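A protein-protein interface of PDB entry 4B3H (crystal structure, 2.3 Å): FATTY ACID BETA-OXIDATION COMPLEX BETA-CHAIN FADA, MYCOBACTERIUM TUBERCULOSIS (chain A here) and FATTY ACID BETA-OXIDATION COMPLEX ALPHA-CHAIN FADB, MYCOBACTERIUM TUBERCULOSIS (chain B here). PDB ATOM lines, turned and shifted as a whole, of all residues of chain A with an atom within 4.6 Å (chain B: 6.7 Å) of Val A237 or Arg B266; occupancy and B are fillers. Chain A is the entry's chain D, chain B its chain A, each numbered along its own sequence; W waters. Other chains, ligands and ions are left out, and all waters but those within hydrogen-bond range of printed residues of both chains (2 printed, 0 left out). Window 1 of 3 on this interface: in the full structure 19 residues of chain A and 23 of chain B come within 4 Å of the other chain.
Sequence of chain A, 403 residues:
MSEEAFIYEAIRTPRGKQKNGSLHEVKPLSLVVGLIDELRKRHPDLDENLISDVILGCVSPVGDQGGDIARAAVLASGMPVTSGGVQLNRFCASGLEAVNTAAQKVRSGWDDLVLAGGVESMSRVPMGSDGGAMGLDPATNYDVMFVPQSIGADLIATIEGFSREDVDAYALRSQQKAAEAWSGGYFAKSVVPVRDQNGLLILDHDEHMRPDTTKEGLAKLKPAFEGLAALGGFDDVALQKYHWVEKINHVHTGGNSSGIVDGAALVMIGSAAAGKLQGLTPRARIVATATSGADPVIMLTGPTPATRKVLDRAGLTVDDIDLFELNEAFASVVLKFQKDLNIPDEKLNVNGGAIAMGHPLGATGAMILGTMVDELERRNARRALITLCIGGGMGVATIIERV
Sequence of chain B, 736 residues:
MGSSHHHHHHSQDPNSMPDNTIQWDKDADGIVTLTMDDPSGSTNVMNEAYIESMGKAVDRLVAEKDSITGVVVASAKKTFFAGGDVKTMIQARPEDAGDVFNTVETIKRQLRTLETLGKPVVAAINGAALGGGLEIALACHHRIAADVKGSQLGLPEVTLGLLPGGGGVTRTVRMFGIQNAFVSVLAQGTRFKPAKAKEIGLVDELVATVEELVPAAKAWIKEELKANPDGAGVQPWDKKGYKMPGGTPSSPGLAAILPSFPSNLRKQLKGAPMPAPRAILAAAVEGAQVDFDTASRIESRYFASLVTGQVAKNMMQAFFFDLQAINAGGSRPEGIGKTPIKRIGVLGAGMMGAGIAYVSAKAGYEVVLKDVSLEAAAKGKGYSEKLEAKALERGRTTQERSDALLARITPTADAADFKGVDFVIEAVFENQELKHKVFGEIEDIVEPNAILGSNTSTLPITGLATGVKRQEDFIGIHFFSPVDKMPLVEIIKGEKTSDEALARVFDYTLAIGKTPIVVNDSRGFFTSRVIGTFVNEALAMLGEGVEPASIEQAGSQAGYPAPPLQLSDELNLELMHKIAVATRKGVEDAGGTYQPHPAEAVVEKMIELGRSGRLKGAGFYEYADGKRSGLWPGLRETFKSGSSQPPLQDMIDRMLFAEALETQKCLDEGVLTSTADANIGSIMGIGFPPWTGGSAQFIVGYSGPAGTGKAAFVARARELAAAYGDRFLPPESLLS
CE2 of Tyr A142 touches O of Pro B262, at 3.8 Å.
Tyr A142 touches Leu B265 (CE2 to CD2, 3.7 Å).
NH1 of Arg B266 touches O of Asp A143 (3.9 Å).
NH1 of Arg B266 touches CG of Met A145, 3.0 Å away.
Gly A233 touches Ser B263.
CD of Lys B267 touches CA of Gly A233, at 3.8 Å.
Phe A234 touches Ser B263 (CE1 to OG, 3.3 Å).
Asp A236 touches Lys B267.
Ser B263 touches Val A237 (O to CG2, 3.7 Å).
Val A237 touches Arg B266.
Hydrophobic or aromatic side chains of chain A that line the printed part of chain B: Tyr A142, Met A145, Phe A234 and Val A237.
Printed residues of chain B that touch a printed residue of chain A: Pro B262, Ser B263, Leu B265, Arg B266, Lys B267, Leu B269, Lys B270 and Gly B271.
Along chain B the printed residues that touch a printed residue of chain A span positions 262 to 271.
Among the printed residues, 15 pairs touch across the chains.
Among the printed residues, no Asp or Glu carboxylate lies within 4 Å of a Lys or Arg side-chain nitrogen of the other chain.
NH1 of Arg B266 sits at hydrogen-bond distance from O of Tyr A142 (2.6 Å).
N of Gly B271 sits close to NE2 of Gln A240 (3.4 Å).
The backbone carbonyl oxygen of Arg B266 is in hydrogen-bond range of the side-chain amide nitrogen of Gln A240 (3.1 Å).
The backbone carbonyl oxygen (O) of Arg B266 sits at hydrogen-bond distance from the backbone NH (N) of Gly B271, at 3.2 Å.
Of the printed residues of chain B, Tyr A142 touches Pro B262 (3.8 Å), Leu B265 (3.7 Å), Arg B266 (2.6 Å) and Leu B269 (3.7 Å).
Printed residues of chain B within 4 Å of Asp A143: Arg B266.
Of the printed residues of chain B, Phe A234 touches Ser B263 (3.3 Å).
Val A237 touches two residues of chain B.
Of the printed residues of chain A, Ser B263 touches Gly A233 (3.8 Å), Phe A234 (3.3 Å) and Val A237 (3.7 Å).
Arg B266 touches five residues of chain A.
Printed residues of chain A within 4 Å of Lys B267: Gly A233 and Asp A236.
The nearest printed residue of chain A that does not touch Arg B266 is Asp A236 (6.0 Å).
Water W1 lies within hydrogen-bond range of the side-chain hydroxyl of Tyr A142 and the backbone carbonyl oxygen of Ala B272.
Water W2 lies within hydrogen-bond range of the side-chain carboxylate of Asp A236 and the backbone carbonyl oxygen of Lys B267.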
ATOM      1  N   TYR A 142       0.632   5.794  25.898  1.00  0.00           N
ATOM      2  CA  TYR A 142       1.942   5.769  25.242  1.00  0.00           C
ATOM      3  C   TYR A 142       1.989   4.775  24.090  1.00  0.00           C
ATOM      4  O   TYR A 142       2.529   5.083  23.031  1.00  0.00           O
ATOM      5  CB  TYR A 142       3.041   5.417  26.245  1.00  0.00           C
ATOM      6  CG  TYR A 142       4.432   5.880  25.853  1.00  0.00           C
ATOM      7  CD1 TYR A 142       5.201   5.166  24.924  1.00  0.00           C
ATOM      8  CD2 TYR A 142       4.987   7.029  26.424  1.00  0.00           C
ATOM      9  CE1 TYR A 142       6.478   5.591  24.573  1.00  0.00           C
ATOM     10  CE2 TYR A 142       6.262   7.458  26.082  1.00  0.00           C
ATOM     11  CZ  TYR A 142       7.006   6.735  25.159  1.00  0.00           C
ATOM     12  OH  TYR A 142       8.269   7.167  24.826  1.00  0.00           O
ATOM     13  N   ASP A 143       1.428   3.589  24.310  1.00  0.00           N
ATOM     14  CA  ASP A 143       1.494   2.505  23.332  1.00  0.00           C
ATOM     15  C   ASP A 143       0.575   2.757  22.142  1.00  0.00           C
ATOM     16  O   ASP A 143       1.046   2.843  21.005  1.00  0.00           O
ATOM     17  CB  ASP A 143       1.212   1.151  23.997  1.00  0.00           C
ATOM     18  CG  ASP A 143       2.334   0.716  24.937  1.00  0.00           C
ATOM     19  OD1 ASP A 143       3.480   1.207  24.787  1.00  0.00           O
ATOM     20  OD2 ASP A 143       2.068  -0.117  25.832  1.00  0.00           O
ATOM     21  N   MET A 145      -0.918   5.258  20.185  1.00  0.00           N
ATOM     22  CA  MET A 145      -0.542   6.664  20.011  1.00  0.00           C
ATOM     23  C   MET A 145      -1.739   7.620  19.980  1.00  0.00           C
ATOM     24  O   MET A 145      -2.233   7.978  18.907  1.00  0.00           O
ATOM     25  CB  MET A 145       0.313   6.819  18.746  1.00  0.00           C
ATOM     26  CG  MET A 145       1.244   5.638  18.487  1.00  0.00           C
ATOM     27  SD  MET A 145       2.261   5.763  17.004  1.00  0.00           S
ATOM     28  CE  MET A 145       3.417   7.058  17.450  1.00  0.00           C
ATOM     29  N   VAL A 147      -3.909  10.687  19.759  1.00  0.00           N
ATOM     30  CA  VAL A 147      -3.813  11.977  19.096  1.00  0.00           C
ATOM     31  C   VAL A 147      -5.222  12.558  18.969  1.00  0.00           C
ATOM     32  O   VAL A 147      -6.115  11.901  18.425  1.00  0.00           O
ATOM     33  CB  VAL A 147      -3.140  11.849  17.705  1.00  0.00           C
ATOM     34  CG1 VAL A 147      -3.408  13.076  16.850  1.00  0.00           C
ATOM     35  CG2 VAL A 147      -1.639  11.640  17.849  1.00  0.00           C
ATOM     36  N   GLY A 233       3.341  18.027  21.658  1.00  0.00           N
ATOM     37  CA  GLY A 233       3.608  16.594  21.607  1.00  0.00           C
ATOM     38  C   GLY A 233       2.901  15.868  20.481  1.00  0.00           C
ATOM     39  O   GLY A 233       3.511  15.055  19.787  1.00  0.00           O
ATOM     40  N   PHE A 234       1.619  16.179  20.293  1.00  0.00           N
ATOM     41  CA  PHE A 234       0.740  15.412  19.402  1.00  0.00           C
ATOM     42  C   PHE A 234       1.122  15.456  17.922  1.00  0.00           C
ATOM     43  O   PHE A 234       0.976  14.456  17.220  1.00  0.00           O
ATOM     44  CB  PHE A 234      -0.722  15.830  19.588  1.00  0.00           C
ATOM     45  CG  PHE A 234      -1.237  15.663  20.994  1.00  0.00           C
ATOM     46  CD1 PHE A 234      -1.336  14.399  21.576  1.00  0.00           C
ATOM     47  CD2 PHE A 234      -1.653  16.773  21.730  1.00  0.00           C
ATOM     48  CE1 PHE A 234      -1.826  14.249  22.867  1.00  0.00           C
ATOM     49  CE2 PHE A 234      -2.141  16.626  23.021  1.00  0.00           C
ATOM     50  CZ  PHE A 234      -2.229  15.365  23.589  1.00  0.00           C
ATOM     51  N   ASP A 235       1.601  16.609  17.453  1.00  0.00           N
ATOM     52  CA  ASP A 235       2.120  16.737  16.088  1.00  0.00           C
ATOM     53  C   ASP A 235       3.289  15.786  15.839  1.00  0.00           C
ATOM     54  O   ASP A 235       3.309  15.068  14.836  1.00  0.00           O
ATOM     55  CB  ASP A 235       2.558  18.177  15.798  1.00  0.00           C
ATOM     56  CG  ASP A 235       1.457  19.012  15.168  1.00  0.00           C
ATOM     57  OD1 ASP A 235       0.314  18.992  15.678  1.00  0.00           O
ATOM     58  OD2 ASP A 235       1.742  19.699  14.163  1.00  0.00           O
ATOM     59  N   ASP A 236       4.255  15.789  16.757  1.00  0.00           N
ATOM     60  CA  ASP A 236       5.430  14.924  16.661  1.00  0.00           C
ATOM     61  C   ASP A 236       5.058  13.449  16.752  1.00  0.00           C
ATOM     62  O   ASP A 236       5.643  12.622  16.055  1.00  0.00           O
ATOM     63  CB  ASP A 236       6.458  15.281  17.739  1.00  0.00           C
ATOM     64  CG  ASP A 236       7.037  16.674  17.557  1.00  0.00           C
ATOM     65  OD1 ASP A 236       6.255  17.640  17.421  1.00  0.00           O
ATOM     66  OD2 ASP A 236       8.278  16.805  17.555  1.00  0.00           O
ATOM     67  N   VAL A 237       4.086  13.131  17.605  1.00  0.00           N
ATOM     68  CA  VAL A 237       3.612  11.757  17.773  1.00  0.00           C
ATOM     69  C   VAL A 237       2.935  11.257  16.494  1.00  0.00           C
ATOM     70  O   VAL A 237       3.186  10.130  16.054  1.00  0.00           O
ATOM     71  CB  VAL A 237       2.656  11.621  18.983  1.00  0.00           C
ATOM     72  CG1 VAL A 237       1.958  10.268  18.987  1.00  0.00           C
ATOM     73  CG2 VAL A 237       3.411  11.824  20.290  1.00  0.00           C
ATOM     74  N   ALA A 238       2.096  12.105  15.899  1.00  0.00           N
ATOM     75  CA  ALA A 238       1.398  11.773  14.659  1.00  0.00           C
ATOM     76  C   ALA A 238       2.381  11.460  13.533  1.00  0.00           C
ATOM     77  O   ALA A 238       2.198  10.487  12.793  1.00  0.00           O
ATOM     78  CB  ALA A 238       0.460  12.901  14.254  1.00  0.00           C
ATOM     79  N   LEU A 239       3.431  12.274  13.426  1.00  0.00           N
ATOM     80  CA  LEU A 239       4.449  12.106  12.391  1.00  0.00           C
ATOM     81  C   LEU A 239       5.413  10.945  12.666  1.00  0.00           C
ATOM     82  O   LEU A 239       6.114  10.495  11.763  1.00  0.00           O
ATOM     83  CB  LEU A 239       5.214  13.416  12.162  1.00  0.00           C
ATOM     84  CG  LEU A 239       4.410  14.600  11.608  1.00  0.00           C
ATOM     85  CD1 LEU A 239       5.262  15.859  11.544  1.00  0.00           C
ATOM     86  CD2 LEU A 239       3.824  14.281  10.241  1.00  0.00           C
ATOM     87  N   GLN A 240       5.444  10.462  13.905  1.00  0.00           N
ATOM     88  CA  GLN A 240       6.206   9.256  14.227  1.00  0.00           C
ATOM     89  C   GLN A 240       5.578   8.024  13.570  1.00  0.00           C
ATOM     90  O   GLN A 240       6.296   7.140  13.094  1.00  0.00           O
ATOM     91  CB  GLN A 240       6.337   9.065  15.741  1.00  0.00           C
ATOM     92  CG  GLN A 240       7.426   9.920  16.379  1.00  0.00           C
ATOM     93  CD  GLN A 240       7.461   9.826  17.898  1.00  0.00           C
ATOM     94  OE1 GLN A 240       7.054   8.822  18.490  1.00  0.00           O
ATOM     95  NE2 GLN A 240       7.964  10.878  18.537  1.00  0.00           N
ATOM     96  N   LYS A 241       4.244   7.974  13.543  1.00  0.00           N
ATOM     97  CA  LYS A 241       3.525   6.912  12.835  1.00  0.00           C
ATOM     98  C   LYS A 241       3.532   7.155  11.332  1.00  0.00           C
ATOM     99  O   LYS A 241       3.833   6.248  10.555  1.00  0.00           O
ATOM    100  CB  LYS A 241       2.084   6.772  13.336  1.00  0.00           C
ATOM    101  CG  LYS A 241       1.350   5.598  12.706  1.00  0.00           C
ATOM    102  CD  LYS A 241       0.125   5.196  13.504  1.00  0.00           C
ATOM    103  CE  LYS A 241      -0.252   3.746  13.234  1.00  0.00           C
ATOM    104  NZ  LYS A 241      -1.202   3.228  14.261  1.00  0.00           N
ATOM    105  N   PHE B 261       0.749  14.257  28.780  1.00  0.00           N
ATOM    106  CA  PHE B 261       2.035  13.914  29.402  1.00  0.00           C
ATOM    107  C   PHE B 261       2.799  12.820  28.646  1.00  0.00           C
ATOM    108  O   PHE B 261       4.005  12.958  28.444  1.00  0.00           O
ATOM    109  CB  PHE B 261       1.892  13.550  30.890  1.00  0.00           C
ATOM    110  CG  PHE B 261       1.524  14.711  31.782  1.00  0.00           C
ATOM    111  CD1 PHE B 261       1.536  16.023  31.312  1.00  0.00           C
ATOM    112  CD2 PHE B 261       1.197  14.487  33.114  1.00  0.00           C
ATOM    113  CE1 PHE B 261       1.198  17.080  32.142  1.00  0.00           C
ATOM    114  CE2 PHE B 261       0.864  15.543  33.951  1.00  0.00           C
ATOM    115  CZ  PHE B 261       0.864  16.841  33.465  1.00  0.00           C
ATOM    116  N   PRO B 262       2.109  11.735  28.223  1.00  0.00           N
ATOM    117  CA  PRO B 262       2.809  10.693  27.460  1.00  0.00           C
ATOM    118  C   PRO B 262       3.253  11.151  26.075  1.00  0.00           C
ATOM    119  O   PRO B 262       4.317  10.737  25.608  1.00  0.00           O
ATOM    120  CB  PRO B 262       1.761   9.577  27.334  1.00  0.00           C
ATOM    121  CG  PRO B 262       0.787   9.839  28.433  1.00  0.00           C
ATOM    122  CD  PRO B 262       0.721  11.332  28.521  1.00  0.00           C
ATOM    123  N   SER B 263       2.446  11.994  25.431  1.00  0.00           N
ATOM    124  CA  SER B 263       2.783  12.532  24.113  1.00  0.00           C
ATOM    125  C   SER B 263       3.967  13.495  24.191  1.00  0.00           C
ATOM    126  O   SER B 263       4.853  13.455  23.338  1.00  0.00           O
ATOM    127  CB  SER B 263       1.574  13.204  23.459  1.00  0.00           C
ATOM    128  OG  SER B 263       1.227  14.405  24.126  1.00  0.00           O
ATOM    129  N   ASN B 264       3.981  14.346  25.220  1.00  0.00           N
ATOM    130  CA  ASN B 264       5.130  15.209  25.497  1.00  0.00           C
ATOM    131  C   ASN B 264       6.411  14.412  25.711  1.00  0.00           C
ATOM    132  O   ASN B 264       7.469  14.791  25.210  1.00  0.00           O
ATOM    133  CB  ASN B 264       4.870  16.118  26.703  1.00  0.00           C
ATOM    134  CG  ASN B 264       4.196  17.428  26.318  1.00  0.00           C
ATOM    135  OD1 ASN B 264       4.693  18.173  25.469  1.00  0.00           O
ATOM    136  ND2 ASN B 264       3.063  17.720  26.952  1.00  0.00           N
ATOM    137  N   LEU B 265       6.306  13.307  26.447  1.00  0.00           N
ATOM    138  CA  LEU B 265       7.445  12.425  26.687  1.00  0.00           C
ATOM    139  C   LEU B 265       7.914  11.766  25.391  1.00  0.00           C
ATOM    140  O   LEU B 265       9.115  11.663  25.139  1.00  0.00           O
ATOM    141  CB  LEU B 265       7.107  11.364  27.743  1.00  0.00           C
ATOM    142  CG  LEU B 265       8.198  10.345  28.111  1.00  0.00           C
ATOM    143  CD1 LEU B 265       9.409  11.014  28.754  1.00  0.00           C
ATOM    144  CD2 LEU B 265       7.638   9.267  29.025  1.00  0.00           C
ATOM    145  N   ARG B 266       6.956  11.333  24.575  1.00  0.00           N
ATOM    146  CA  ARG B 266       7.252  10.685  23.303  1.00  0.00           C
ATOM    147  C   ARG B 266       7.912  11.654  22.327  1.00  0.00           C
ATOM    148  O   ARG B 266       8.774  11.257  21.543  1.00  0.00           O
ATOM    149  CB  ARG B 266       5.978  10.095  22.699  1.00  0.00           C
ATOM    150  CG  ARG B 266       6.244   8.970  21.720  1.00  0.00           C
ATOM    151  CD  ARG B 266       5.011   8.119  21.493  1.00  0.00           C
ATOM    152  NE  ARG B 266       5.374   6.823  20.927  1.00  0.00           N
ATOM    153  CZ  ARG B 266       4.503   5.876  20.597  1.00  0.00           C
ATOM    154  NH1 ARG B 266       3.201   6.078  20.767  1.00  0.00           N
ATOM    155  NH2 ARG B 266       4.931   4.725  20.093  1.00  0.00           N
ATOM    156  N   LYS B 267       7.494  12.918  22.391  1.00  0.00           N
ATOM    157  CA  LYS B 267       8.113  14.015  21.646  1.00  0.00           C
ATOM    158  C   LYS B 267       9.576  14.202  22.066  1.00  0.00           C
ATOM    159  O   LYS B 267      10.463  14.254  21.211  1.00  0.00           O
ATOM    160  CB  LYS B 267       7.316  15.306  21.872  1.00  0.00           C
ATOM    161  CG  LYS B 267       7.843  16.550  21.170  1.00  0.00           C
ATOM    162  CD  LYS B 267       7.165  17.789  21.739  1.00  0.00           C
ATOM    163  CE  LYS B 267       7.058  18.914  20.721  1.00  0.00           C
ATOM    164  NZ  LYS B 267       8.304  19.720  20.616  1.00  0.00           N
ATOM    165  N   GLN B 268       9.813  14.287  23.377  1.00  0.00           N
ATOM    166  CA  GLN B 268      11.159  14.474  23.932  1.00  0.00           C
ATOM    167  C   GLN B 268      12.098  13.335  23.548  1.00  0.00           C
ATOM    168  O   GLN B 268      13.254  13.575  23.207  1.00  0.00           O
ATOM    169  CB  GLN B 268      11.123  14.612  25.461  1.00  0.00           C
ATOM    170  CG  GLN B 268      10.319  15.790  26.003  1.00  0.00           C
ATOM    171  CD  GLN B 268      10.965  17.145  25.742  1.00  0.00           C
ATOM    172  OE1 GLN B 268      10.926  17.666  24.623  1.00  0.00           O
ATOM    173  NE2 GLN B 268      11.542  17.736  26.788  1.00  0.00           N
ATOM    174  N   LEU B 269      11.592  12.103  23.597  1.00  0.00           N
ATOM    175  CA  LEU B 269      12.395  10.918  23.287  1.00  0.00           C
ATOM    176  C   LEU B 269      12.421  10.577  21.790  1.00  0.00           C
ATOM    177  O   LEU B 269      13.146   9.676  21.373  1.00  0.00           O
ATOM    178  CB  LEU B 269      11.924   9.708  24.106  1.00  0.00           C
ATOM    179  CG  LEU B 269      11.951   9.786  25.638  1.00  0.00           C
ATOM    180  CD1 LEU B 269      11.393   8.504  26.235  1.00  0.00           C
ATOM    181  CD2 LEU B 269      13.350  10.065  26.180  1.00  0.00           C
ATOM    182  N   LYS B 270      11.623  11.297  21.000  1.00  0.00           N
ATOM    183  CA  LYS B 270      11.578  11.154  19.534  1.00  0.00           C
ATOM    184  C   LYS B 270      11.154   9.766  19.052  1.00  0.00           C
ATOM    185  O   LYS B 270      11.469   9.372  17.930  1.00  0.00           O
ATOM    186  CB  LYS B 270      12.920  11.555  18.904  1.00  0.00           C
ATOM    187  CG  LYS B 270      13.246  13.033  19.036  1.00  0.00           C
ATOM    188  CD  LYS B 270      14.720  13.303  18.800  1.00  0.00           C
ATOM    189  CE  LYS B 270      15.046  14.769  19.037  1.00  0.00           C
ATOM    190  NZ  LYS B 270      16.503  15.028  18.864  1.00  0.00           N
ATOM    191  N   GLY B 271      10.440   9.032  19.901  1.00  0.00           N
ATOM    192  CA  GLY B 271       9.991   7.686  19.570  1.00  0.00           C
ATOM    193  C   GLY B 271      11.019   6.587  19.785  1.00  0.00           C
ATOM    194  O   GLY B 271      10.808   5.455  19.354  1.00  0.00           O
ATOM    195  N   ALA B 272      12.128   6.911  20.450  1.00  0.00           N
ATOM    196  CA  ALA B 272      13.171   5.921  20.750  1.00  0.00           C
ATOM    197  C   ALA B 272      12.674   4.883  21.761  1.00  0.00           C
ATOM    198  O   ALA B 272      11.914   5.225  22.673  1.00  0.00           O
ATOM    199  CB  ALA B 272      14.432   6.604  21.263  1.00  0.00           C
HETATM  200  O   HOH W   1       9.606   6.886  22.597  1.00  0.00           O
HETATM  201  O   HOH W   2      10.202  14.953  18.308  1.00  0.00           O
